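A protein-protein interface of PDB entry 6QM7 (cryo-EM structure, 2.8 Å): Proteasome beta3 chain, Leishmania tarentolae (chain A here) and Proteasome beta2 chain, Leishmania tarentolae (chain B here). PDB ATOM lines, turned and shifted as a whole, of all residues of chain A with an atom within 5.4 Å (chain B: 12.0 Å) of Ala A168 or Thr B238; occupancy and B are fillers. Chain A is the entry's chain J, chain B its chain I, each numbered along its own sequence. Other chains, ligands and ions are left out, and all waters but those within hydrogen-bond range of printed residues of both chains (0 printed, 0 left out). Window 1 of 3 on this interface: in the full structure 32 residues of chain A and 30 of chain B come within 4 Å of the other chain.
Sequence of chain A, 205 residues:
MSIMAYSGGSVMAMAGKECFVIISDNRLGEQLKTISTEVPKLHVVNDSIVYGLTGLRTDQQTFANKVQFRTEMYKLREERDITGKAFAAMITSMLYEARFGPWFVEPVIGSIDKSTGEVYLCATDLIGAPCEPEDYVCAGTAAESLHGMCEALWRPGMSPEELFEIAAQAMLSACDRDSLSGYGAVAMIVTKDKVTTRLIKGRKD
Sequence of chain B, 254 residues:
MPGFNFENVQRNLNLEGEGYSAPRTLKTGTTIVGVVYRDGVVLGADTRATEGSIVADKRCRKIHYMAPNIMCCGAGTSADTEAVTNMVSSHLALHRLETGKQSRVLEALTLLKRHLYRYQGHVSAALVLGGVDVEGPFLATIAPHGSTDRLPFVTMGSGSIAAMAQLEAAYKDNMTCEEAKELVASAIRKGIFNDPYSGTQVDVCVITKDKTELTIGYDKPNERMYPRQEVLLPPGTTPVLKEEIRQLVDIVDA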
ATOM      1  N   MET A  12     -21.291  17.380  -5.525  1.00  0.00           N
ATOM      2  CA  MET A  12     -20.482  16.201  -5.871  1.00  0.00           C
ATOM      3  C   MET A  12     -19.254  16.199  -4.974  1.00  0.00           C
ATOM      4  O   MET A  12     -18.787  17.287  -4.636  1.00  0.00           O
ATOM      5  CB  MET A  12     -20.092  16.252  -7.344  1.00  0.00           C
ATOM      6  CG  MET A  12     -19.354  15.023  -7.809  1.00  0.00           C
ATOM      7  SD  MET A  12     -17.599  15.375  -7.989  1.00  0.00           S
ATOM      8  CE  MET A  12     -17.694  16.466  -9.407  1.00  0.00           C
ATOM      9  N   ILE A  23     -17.701  19.805  -4.182  1.00  0.00           N
ATOM     10  CA  ILE A  23     -17.973  20.962  -5.075  1.00  0.00           C
ATOM     11  C   ILE A  23     -19.482  21.090  -5.243  1.00  0.00           C
ATOM     12  O   ILE A  23     -20.121  20.090  -5.599  1.00  0.00           O
ATOM     13  CB  ILE A  23     -17.223  20.768  -6.396  1.00  0.00           C
ATOM     14  CG1 ILE A  23     -17.448  21.937  -7.347  1.00  0.00           C
ATOM     15  CG2 ILE A  23     -17.570  19.447  -7.067  1.00  0.00           C
ATOM     16  CD1 ILE A  23     -16.532  21.892  -8.557  1.00  0.00           C
ATOM     17  N   LEU A 163      -7.240  16.328  -8.836  1.00  0.00           N
ATOM     18  CA  LEU A 163      -8.605  15.920  -8.408  1.00  0.00           C
ATOM     19  C   LEU A 163      -9.542  17.113  -8.565  1.00  0.00           C
ATOM     20  O   LEU A 163     -10.658  16.922  -9.054  1.00  0.00           O
ATOM     21  CB  LEU A 163      -8.595  15.461  -6.941  1.00  0.00           C
ATOM     22  CG  LEU A 163      -9.512  14.296  -6.555  1.00  0.00           C
ATOM     23  CD1 LEU A 163      -9.979  14.462  -5.122  1.00  0.00           C
ATOM     24  CD2 LEU A 163     -10.725  14.114  -7.468  1.00  0.00           C
ATOM     25  N   PHE A 164      -9.098  18.286  -8.116  1.00  0.00           N
ATOM     26  CA  PHE A 164      -9.839  19.565  -8.228  1.00  0.00           C
ATOM     27  C   PHE A 164     -10.243  19.799  -9.684  1.00  0.00           C
ATOM     28  O   PHE A 164     -11.419  20.093  -9.938  1.00  0.00           O
ATOM     29  CB  PHE A 164      -9.008  20.748  -7.735  1.00  0.00           C
ATOM     30  CG  PHE A 164      -9.638  22.058  -8.107  1.00  0.00           C
ATOM     31  CD1 PHE A 164     -10.795  22.484  -7.480  1.00  0.00           C
ATOM     32  CD2 PHE A 164      -9.135  22.811  -9.150  1.00  0.00           C
ATOM     33  CE1 PHE A 164     -11.408  23.667  -7.860  1.00  0.00           C
ATOM     34  CE2 PHE A 164      -9.745  24.001  -9.519  1.00  0.00           C
ATOM     35  CZ  PHE A 164     -10.884  24.424  -8.879  1.00  0.00           C
ATOM     36  N   GLU A 165      -9.284  19.671 -10.599  1.00  0.00           N
ATOM     37  CA  GLU A 165      -9.483  19.966 -12.036  1.00  0.00           C
ATOM     38  C   GLU A 165     -10.590  19.082 -12.595  1.00  0.00           C
ATOM     39  O   GLU A 165     -11.503  19.636 -13.220  1.00  0.00           O
ATOM     40  CB  GLU A 165      -8.189  19.795 -12.819  1.00  0.00           C
ATOM     41  CG  GLU A 165      -7.184  20.882 -12.505  1.00  0.00           C
ATOM     42  CD  GLU A 165      -7.686  22.309 -12.677  1.00  0.00           C
ATOM     43  OE1 GLU A 165      -7.241  23.208 -11.913  1.00  0.00           O
ATOM     44  OE2 GLU A 165      -8.517  22.526 -13.583  1.00  0.00           O
ATOM     45  N   ILE A 166     -10.550  17.781 -12.337  1.00  0.00           N
ATOM     46  CA  ILE A 166     -11.545  16.855 -12.942  1.00  0.00           C
ATOM     47  C   ILE A 166     -12.906  17.047 -12.263  1.00  0.00           C
ATOM     48  O   ILE A 166     -13.917  16.861 -12.960  1.00  0.00           O
ATOM     49  CB  ILE A 166     -11.067  15.395 -12.940  1.00  0.00           C
ATOM     50  CG1 ILE A 166     -11.146  14.753 -11.557  1.00  0.00           C
ATOM     51  CG2 ILE A 166      -9.683  15.275 -13.561  1.00  0.00           C
ATOM     52  CD1 ILE A 166     -12.201  13.698 -11.485  1.00  0.00           C
ATOM     53  N   ALA A 167     -12.939  17.436 -10.983  1.00  0.00           N
ATOM     54  CA  ALA A 167     -14.192  17.686 -10.231  1.00  0.00           C
ATOM     55  C   ALA A 167     -14.815  18.983 -10.739  1.00  0.00           C
ATOM     56  O   ALA A 167     -16.027  19.002 -10.941  1.00  0.00           O
ATOM     57  CB  ALA A 167     -13.952  17.736  -8.741  1.00  0.00           C
ATOM     58  N   ALA A 168     -14.011  20.023 -10.948  1.00  0.00           N
ATOM     59  CA  ALA A 168     -14.469  21.317 -11.497  1.00  0.00           C
ATOM     60  C   ALA A 168     -15.036  21.084 -12.900  1.00  0.00           C
ATOM     61  O   ALA A 168     -16.189  21.484 -13.134  1.00  0.00           O
ATOM     62  CB  ALA A 168     -13.348  22.315 -11.506  1.00  0.00           C
ATOM     63  N   GLN A 169     -14.277  20.407 -13.766  1.00  0.00           N
ATOM     64  CA  GLN A 169     -14.678  20.095 -15.164  1.00  0.00           C
ATOM     65  C   GLN A 169     -15.934  19.238 -15.175  1.00  0.00           C
ATOM     66  O   GLN A 169     -16.738  19.405 -16.096  1.00  0.00           O
ATOM     67  CB  GLN A 169     -13.582  19.336 -15.919  1.00  0.00           C
ATOM     68  CG  GLN A 169     -12.383  20.195 -16.312  1.00  0.00           C
ATOM     69  CD  GLN A 169     -12.835  21.499 -16.903  1.00  0.00           C
ATOM     70  OE1 GLN A 169     -13.643  21.508 -17.826  1.00  0.00           O
ATOM     71  NE2 GLN A 169     -12.348  22.594 -16.343  1.00  0.00           N
ATOM     72  N   ALA A 170     -16.067  18.325 -14.220  1.00  0.00           N
ATOM     73  CA  ALA A 170     -17.282  17.497 -14.049  1.00  0.00           C
ATOM     74  C   ALA A 170     -18.430  18.410 -13.656  1.00  0.00           C
ATOM     75  O   ALA A 170     -19.441  18.422 -14.370  1.00  0.00           O
ATOM     76  CB  ALA A 170     -17.088  16.418 -13.019  1.00  0.00           C
ATOM     77  N   MET A 171     -18.272  19.148 -12.566  1.00  0.00           N
ATOM     78  CA  MET A 171     -19.384  19.958 -12.024  1.00  0.00           C
ATOM     79  C   MET A 171     -19.834  20.937 -13.107  1.00  0.00           C
ATOM     80  O   MET A 171     -21.040  21.005 -13.342  1.00  0.00           O
ATOM     81  CB  MET A 171     -19.010  20.722 -10.750  1.00  0.00           C
ATOM     82  CG  MET A 171     -20.173  21.519 -10.172  1.00  0.00           C
ATOM     83  SD  MET A 171     -21.719  20.563 -10.031  1.00  0.00           S
ATOM     84  CE  MET A 171     -21.577  20.017  -8.329  1.00  0.00           C
ATOM     85  N   LEU A 172     -18.904  21.640 -13.752  1.00  0.00           N
ATOM     86  CA  LEU A 172     -19.236  22.666 -14.769  1.00  0.00           C
ATOM     87  C   LEU A 172     -19.903  22.019 -15.979  1.00  0.00           C
ATOM     88  O   LEU A 172     -20.940  22.535 -16.415  1.00  0.00           O
ATOM     89  CB  LEU A 172     -17.977  23.402 -15.203  1.00  0.00           C
ATOM     90  CG  LEU A 172     -17.366  24.334 -14.161  1.00  0.00           C
ATOM     91  CD1 LEU A 172     -16.062  24.915 -14.695  1.00  0.00           C
ATOM     92  CD2 LEU A 172     -18.342  25.435 -13.773  1.00  0.00           C
ATOM     93  N   SER A 173     -19.332  20.957 -16.528  1.00  0.00           N
ATOM     94  CA  SER A 173     -19.858  20.313 -17.756  1.00  0.00           C
ATOM     95  C   SER A 173     -21.260  19.767 -17.497  1.00  0.00           C
ATOM     96  O   SER A 173     -22.105  19.902 -18.384  1.00  0.00           O
ATOM     97  CB  SER A 173     -18.920  19.254 -18.253  1.00  0.00           C
ATOM     98  OG  SER A 173     -17.658  19.839 -18.570  1.00  0.00           O
ATOM     99  N   ILE A 200     -15.247  28.883  -8.642  1.00  0.00           N
ATOM    100  CA  ILE A 200     -14.931  28.480 -10.041  1.00  0.00           C
ATOM    101  C   ILE A 200     -15.813  29.299 -10.981  1.00  0.00           C
ATOM    102  O   ILE A 200     -17.033  29.321 -10.779  1.00  0.00           O
ATOM    103  CB  ILE A 200     -15.176  26.970 -10.203  1.00  0.00           C
ATOM    104  CG1 ILE A 200     -14.223  26.153  -9.337  1.00  0.00           C
ATOM    105  CG2 ILE A 200     -15.105  26.531 -11.650  1.00  0.00           C
ATOM    106  CD1 ILE A 200     -14.802  24.814  -8.941  1.00  0.00           C
ATOM    107  N   VAL B 231      -7.648  10.963 -19.281  1.00  0.00           N
ATOM    108  CA  VAL B 231      -7.780  12.359 -19.799  1.00  0.00           C
ATOM    109  C   VAL B 231      -7.019  13.279 -18.842  1.00  0.00           C
ATOM    110  O   VAL B 231      -7.422  13.341 -17.662  1.00  0.00           O
ATOM    111  CB  VAL B 231      -9.258  12.786 -19.934  1.00  0.00           C
ATOM    112  CG1 VAL B 231      -9.399  14.274 -20.245  1.00  0.00           C
ATOM    113  CG2 VAL B 231     -10.000  11.947 -20.968  1.00  0.00           C
ATOM    114  N   LEU B 232      -5.976  13.961 -19.334  1.00  0.00           N
ATOM    115  CA  LEU B 232      -5.052  14.788 -18.508  1.00  0.00           C
ATOM    116  C   LEU B 232      -5.470  16.263 -18.588  1.00  0.00           C
ATOM    117  O   LEU B 232      -5.426  16.848 -19.692  1.00  0.00           O
ATOM    118  CB  LEU B 232      -3.594  14.574 -18.940  1.00  0.00           C
ATOM    119  CG  LEU B 232      -2.763  13.683 -18.007  1.00  0.00           C
ATOM    120  CD1 LEU B 232      -3.032  12.204 -18.266  1.00  0.00           C
ATOM    121  CD2 LEU B 232      -1.274  13.991 -18.123  1.00  0.00           C
ATOM    122  N   LEU B 233      -5.874  16.804 -17.433  1.00  0.00           N
ATOM    123  CA  LEU B 233      -6.263  18.218 -17.199  1.00  0.00           C
ATOM    124  C   LEU B 233      -5.244  18.835 -16.242  1.00  0.00           C
ATOM    125  O   LEU B 233      -5.388  18.721 -15.024  1.00  0.00           O
ATOM    126  CB  LEU B 233      -7.684  18.243 -16.622  1.00  0.00           C
ATOM    127  CG  LEU B 233      -8.744  17.515 -17.448  1.00  0.00           C
ATOM    128  CD1 LEU B 233     -10.090  17.510 -16.734  1.00  0.00           C
ATOM    129  CD2 LEU B 233      -8.870  18.126 -18.838  1.00  0.00           C
ATOM    130  N   PRO B 234      -4.164  19.477 -16.751  1.00  0.00           N
ATOM    131  CA  PRO B 234      -3.101  19.986 -15.882  1.00  0.00           C
ATOM    132  C   PRO B 234      -3.580  21.135 -14.995  1.00  0.00           C
ATOM    133  O   PRO B 234      -4.417  21.924 -15.420  1.00  0.00           O
ATOM    134  CB  PRO B 234      -2.021  20.458 -16.868  1.00  0.00           C
ATOM    135  CG  PRO B 234      -2.793  20.781 -18.133  1.00  0.00           C
ATOM    136  CD  PRO B 234      -3.913  19.762 -18.174  1.00  0.00           C
ATOM    137  N   PRO B 235      -3.081  21.264 -13.742  1.00  0.00           N
ATOM    138  CA  PRO B 235      -3.472  22.366 -12.854  1.00  0.00           C
ATOM    139  C   PRO B 235      -3.512  23.756 -13.515  1.00  0.00           C
ATOM    140  O   PRO B 235      -2.612  24.065 -14.282  1.00  0.00           O
ATOM    141  CB  PRO B 235      -2.385  22.323 -11.770  1.00  0.00           C
ATOM    142  CG  PRO B 235      -2.048  20.849 -11.675  1.00  0.00           C
ATOM    143  CD  PRO B 235      -2.132  20.341 -13.099  1.00  0.00           C
ATOM    144  N   GLY B 236      -4.554  24.543 -13.210  1.00  0.00           N
ATOM    145  CA  GLY B 236      -4.841  25.848 -13.838  1.00  0.00           C
ATOM    146  C   GLY B 236      -5.611  25.712 -15.146  1.00  0.00           C
ATOM    147  O   GLY B 236      -5.763  26.731 -15.851  1.00  0.00           O
ATOM    148  N   THR B 237      -6.075  24.500 -15.469  1.00  0.00           N
ATOM    149  CA  THR B 237      -6.978  24.204 -16.614  1.00  0.00           C
ATOM    150  C   THR B 237      -8.310  24.910 -16.374  1.00  0.00           C
ATOM    151  O   THR B 237      -8.752  25.640 -17.271  1.00  0.00           O
ATOM    152  CB  THR B 237      -7.141  22.692 -16.823  1.00  0.00           C
ATOM    153  OG1 THR B 237      -6.026  22.273 -17.609  1.00  0.00           O
ATOM    154  CG2 THR B 237      -8.420  22.292 -17.529  1.00  0.00           C
ATOM    155  N   THR B 238      -8.911  24.693 -15.204  1.00  0.00           N
ATOM    156  CA  THR B 238     -10.215  25.272 -14.800  1.00  0.00           C
ATOM    157  C   THR B 238      -9.973  26.681 -14.267  1.00  0.00           C
ATOM    158  O   THR B 238      -9.207  26.837 -13.317  1.00  0.00           O
ATOM    159  CB  THR B 238     -10.924  24.394 -13.762  1.00  0.00           C
ATOM    160  OG1 THR B 238     -10.940  23.040 -14.221  1.00  0.00           O
ATOM    161  CG2 THR B 238     -12.339  24.855 -13.487  1.00  0.00           C
ATOM    162  N   PRO B 239     -10.617  27.728 -14.850  1.00  0.00           N
ATOM    163  CA  PRO B 239     -10.447  29.108 -14.387  1.00  0.00           C
ATOM    164  C   PRO B 239     -11.126  29.382 -13.034  1.00  0.00           C
ATOM    165  O   PRO B 239     -12.272  29.032 -12.857  1.00  0.00           O
ATOM    166  CB  PRO B 239     -11.082  29.955 -15.499  1.00  0.00           C
ATOM    167  CG  PRO B 239     -12.108  29.042 -16.126  1.00  0.00           C
ATOM    168  CD  PRO B 239     -11.537  27.647 -15.998  1.00  0.00           C
ATOM    169  N   VAL B 240     -10.380  30.019 -12.130  1.00  0.00           N
ATOM    170  CA  VAL B 240     -10.712  30.199 -10.689  1.00  0.00           C
ATOM    171  C   VAL B 240     -10.746  31.700 -10.385  1.00  0.00           C
ATOM    172  O   VAL B 240      -9.716  32.369 -10.567  1.00  0.00           O
ATOM    173  CB  VAL B 240      -9.688  29.462  -9.805  1.00  0.00           C
ATOM    174  CG1 VAL B 240      -9.781  29.881  -8.349  1.00  0.00           C
ATOM    175  CG2 VAL B 240      -9.822  27.954  -9.924  1.00  0.00           C
ATOM    176  N   LEU B 241     -11.888  32.184  -9.901  1.00  0.00           N
ATOM    177  CA  LEU B 241     -12.124  33.605  -9.562  1.00  0.00           C
ATOM    178  C   LEU B 241     -11.445  33.932  -8.231  1.00  0.00           C
ATOM    179  O   LEU B 241     -10.681  34.910  -8.193  1.00  0.00           O
ATOM    180  CB  LEU B 241     -13.633  33.844  -9.487  1.00  0.00           C
ATOM    181  CG  LEU B 241     -14.401  33.579 -10.780  1.00  0.00           C
ATOM    182  CD1 LEU B 241     -15.902  33.736 -10.555  1.00  0.00           C
ATOM    183  CD2 LEU B 241     -13.912  34.498 -11.898  1.00  0.00           C
ATOM    184  N   LYS B 242     -11.724  33.150  -7.186  1.00  0.00           N
ATOM    185  CA  LYS B 242     -11.192  33.361  -5.812  1.00  0.00           C
ATOM    186  C   LYS B 242     -10.693  32.037  -5.238  1.00  0.00           C
ATOM    187  O   LYS B 242     -11.122  30.976  -5.718  1.00  0.00           O
ATOM    188  CB  LYS B 242     -12.266  33.956  -4.901  1.00  0.00           C
ATOM    189  CG  LYS B 242     -12.498  35.447  -5.088  1.00  0.00           C
ATOM    190  CD  LYS B 242     -13.789  35.946  -4.472  1.00  0.00           C
ATOM    191  CE  LYS B 242     -14.465  37.017  -5.305  1.00  0.00           C
ATOM    192  NZ  LYS B 242     -15.864  37.248  -4.867  1.00  0.00           N
ATOM    193  N   GLU B 243      -9.819  32.125  -4.239  1.00  0.00           N
ATOM    194  CA  GLU B 243      -9.143  30.972  -3.600  1.00  0.00           C
ATOM    195  C   GLU B 243      -8.792  31.362  -2.163  1.00  0.00           C
ATOM    196  O   GLU B 243      -8.052  32.344  -1.999  1.00  0.00           O
ATOM    197  CB  GLU B 243      -7.903  30.602  -4.413  1.00  0.00           C
ATOM    198  CG  GLU B 243      -7.104  29.439  -3.840  1.00  0.00           C
ATOM    199  CD  GLU B 243      -5.953  28.952  -4.713  1.00  0.00           C
ATOM    200  OE1 GLU B 243      -6.093  28.975  -5.964  1.00  0.00           O
ATOM    201  OE2 GLU B 243      -4.919  28.532  -4.144  1.00  0.00           O
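The side-chain hydroxyl (OG1) of Thr B238 is in hydrogen-bond range of the side-chain amide nitrogen (NE2) of Gln A169, at 2.6 Å. The side-chain carboxylate (OE1) of Glu A165 is in hydrogen-bond range of the backbone NH (N) of Gly B236 (3.3 Å). The side-chain carboxylate (OE2) of Glu A165 sits at hydrogen-bond distance from the side-chain hydroxyl (OG1) of Thr B238.
OG1 of Thr B237 lies within hydrogen-bond range of O of Pro B234 (2.7 Å). The backbone carbonyl oxygen (O) of Gln A169 is in hydrogen-bond range of the side-chain hydroxyl (OG) of Ser A173 (2.7 Å).
Val B240 touches Phe A164 (CG2 to CZ, 3.8 Å). O of Leu B233 touches CB of Glu A165, at 3.7 Å. Pro B235 touches Glu A165. OE2 of Glu A165 touches CB of Thr B237 (3.5 Å). CG2 of Ile A166 touches CD1 of Leu B233, 3.9 Å away. Ala A168 touches Thr B238. CG of Gln A169 touches CD1 of Leu B233, at 3.6 Å. Leu A172 touches Thr B238. CG2 of Thr B238 touches CG2 of Ile A200, at 3.7 Å. CA of Ile A200 touches O of Pro B239, at 3.9 Å.
Of chain B, only Thr B238 comes within 4 Å of Ala A168. Thr B238 touches just these residues of chain A: Glu A165, Ala A168, Gln A169, Leu A172 and Ile A200. Phe A164 touches just one residue of chain B: Val B240 (3.8 Å). Glu A165 touches just these residues of chain B: Leu B233 (3.7 Å), Pro B235 (3.97 Å), Gly B236 (3.3 Å), Thr B237 (3.5 Å) and Thr B238 (2.6 Å). Ile A166 touches one residue of chain B. Gln A169 touches just these residues of chain B: Leu B233 and Thr B238. Met A171 touches none of the printed residues of chain B. Of the printed residues of chain B, Leu A172 touches Thr B238. Ile A200 touches just these residues of chain B: Thr B238 (3.7 Å) and Pro B239 (3.9 Å). Printed residues of chain A within 4 Å of Leu B233: Glu A165 (3.7 Å), Ile A166 (3.9 Å) and Gln A169 (3.6 Å). Of the printed residues of chain A, Val B240 touches Phe A164. Leu B241 touches none of the printed residues of chain A. The nearest residue of chain B that does not touch Ala A168 is Val B240 (6.8 Å). The nearest residue of chain A that does not touch Thr B238 is Phe A164 (4.4 Å). The nearest printed residue of chain A that does not touch Leu B233 is Ala A167 (6.4 Å).
Printed residues of chain A that touch a printed residue of chain B: Phe A164, Glu A165, Ile A166, Ala A168, Gln A169, Leu A172 and Ile A200. Hydrophobic or aromatic side chains of chain A that line the printed part of chain B: Phe A164, Ile A166, Ala A168, Leu A172 and Ile A200.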
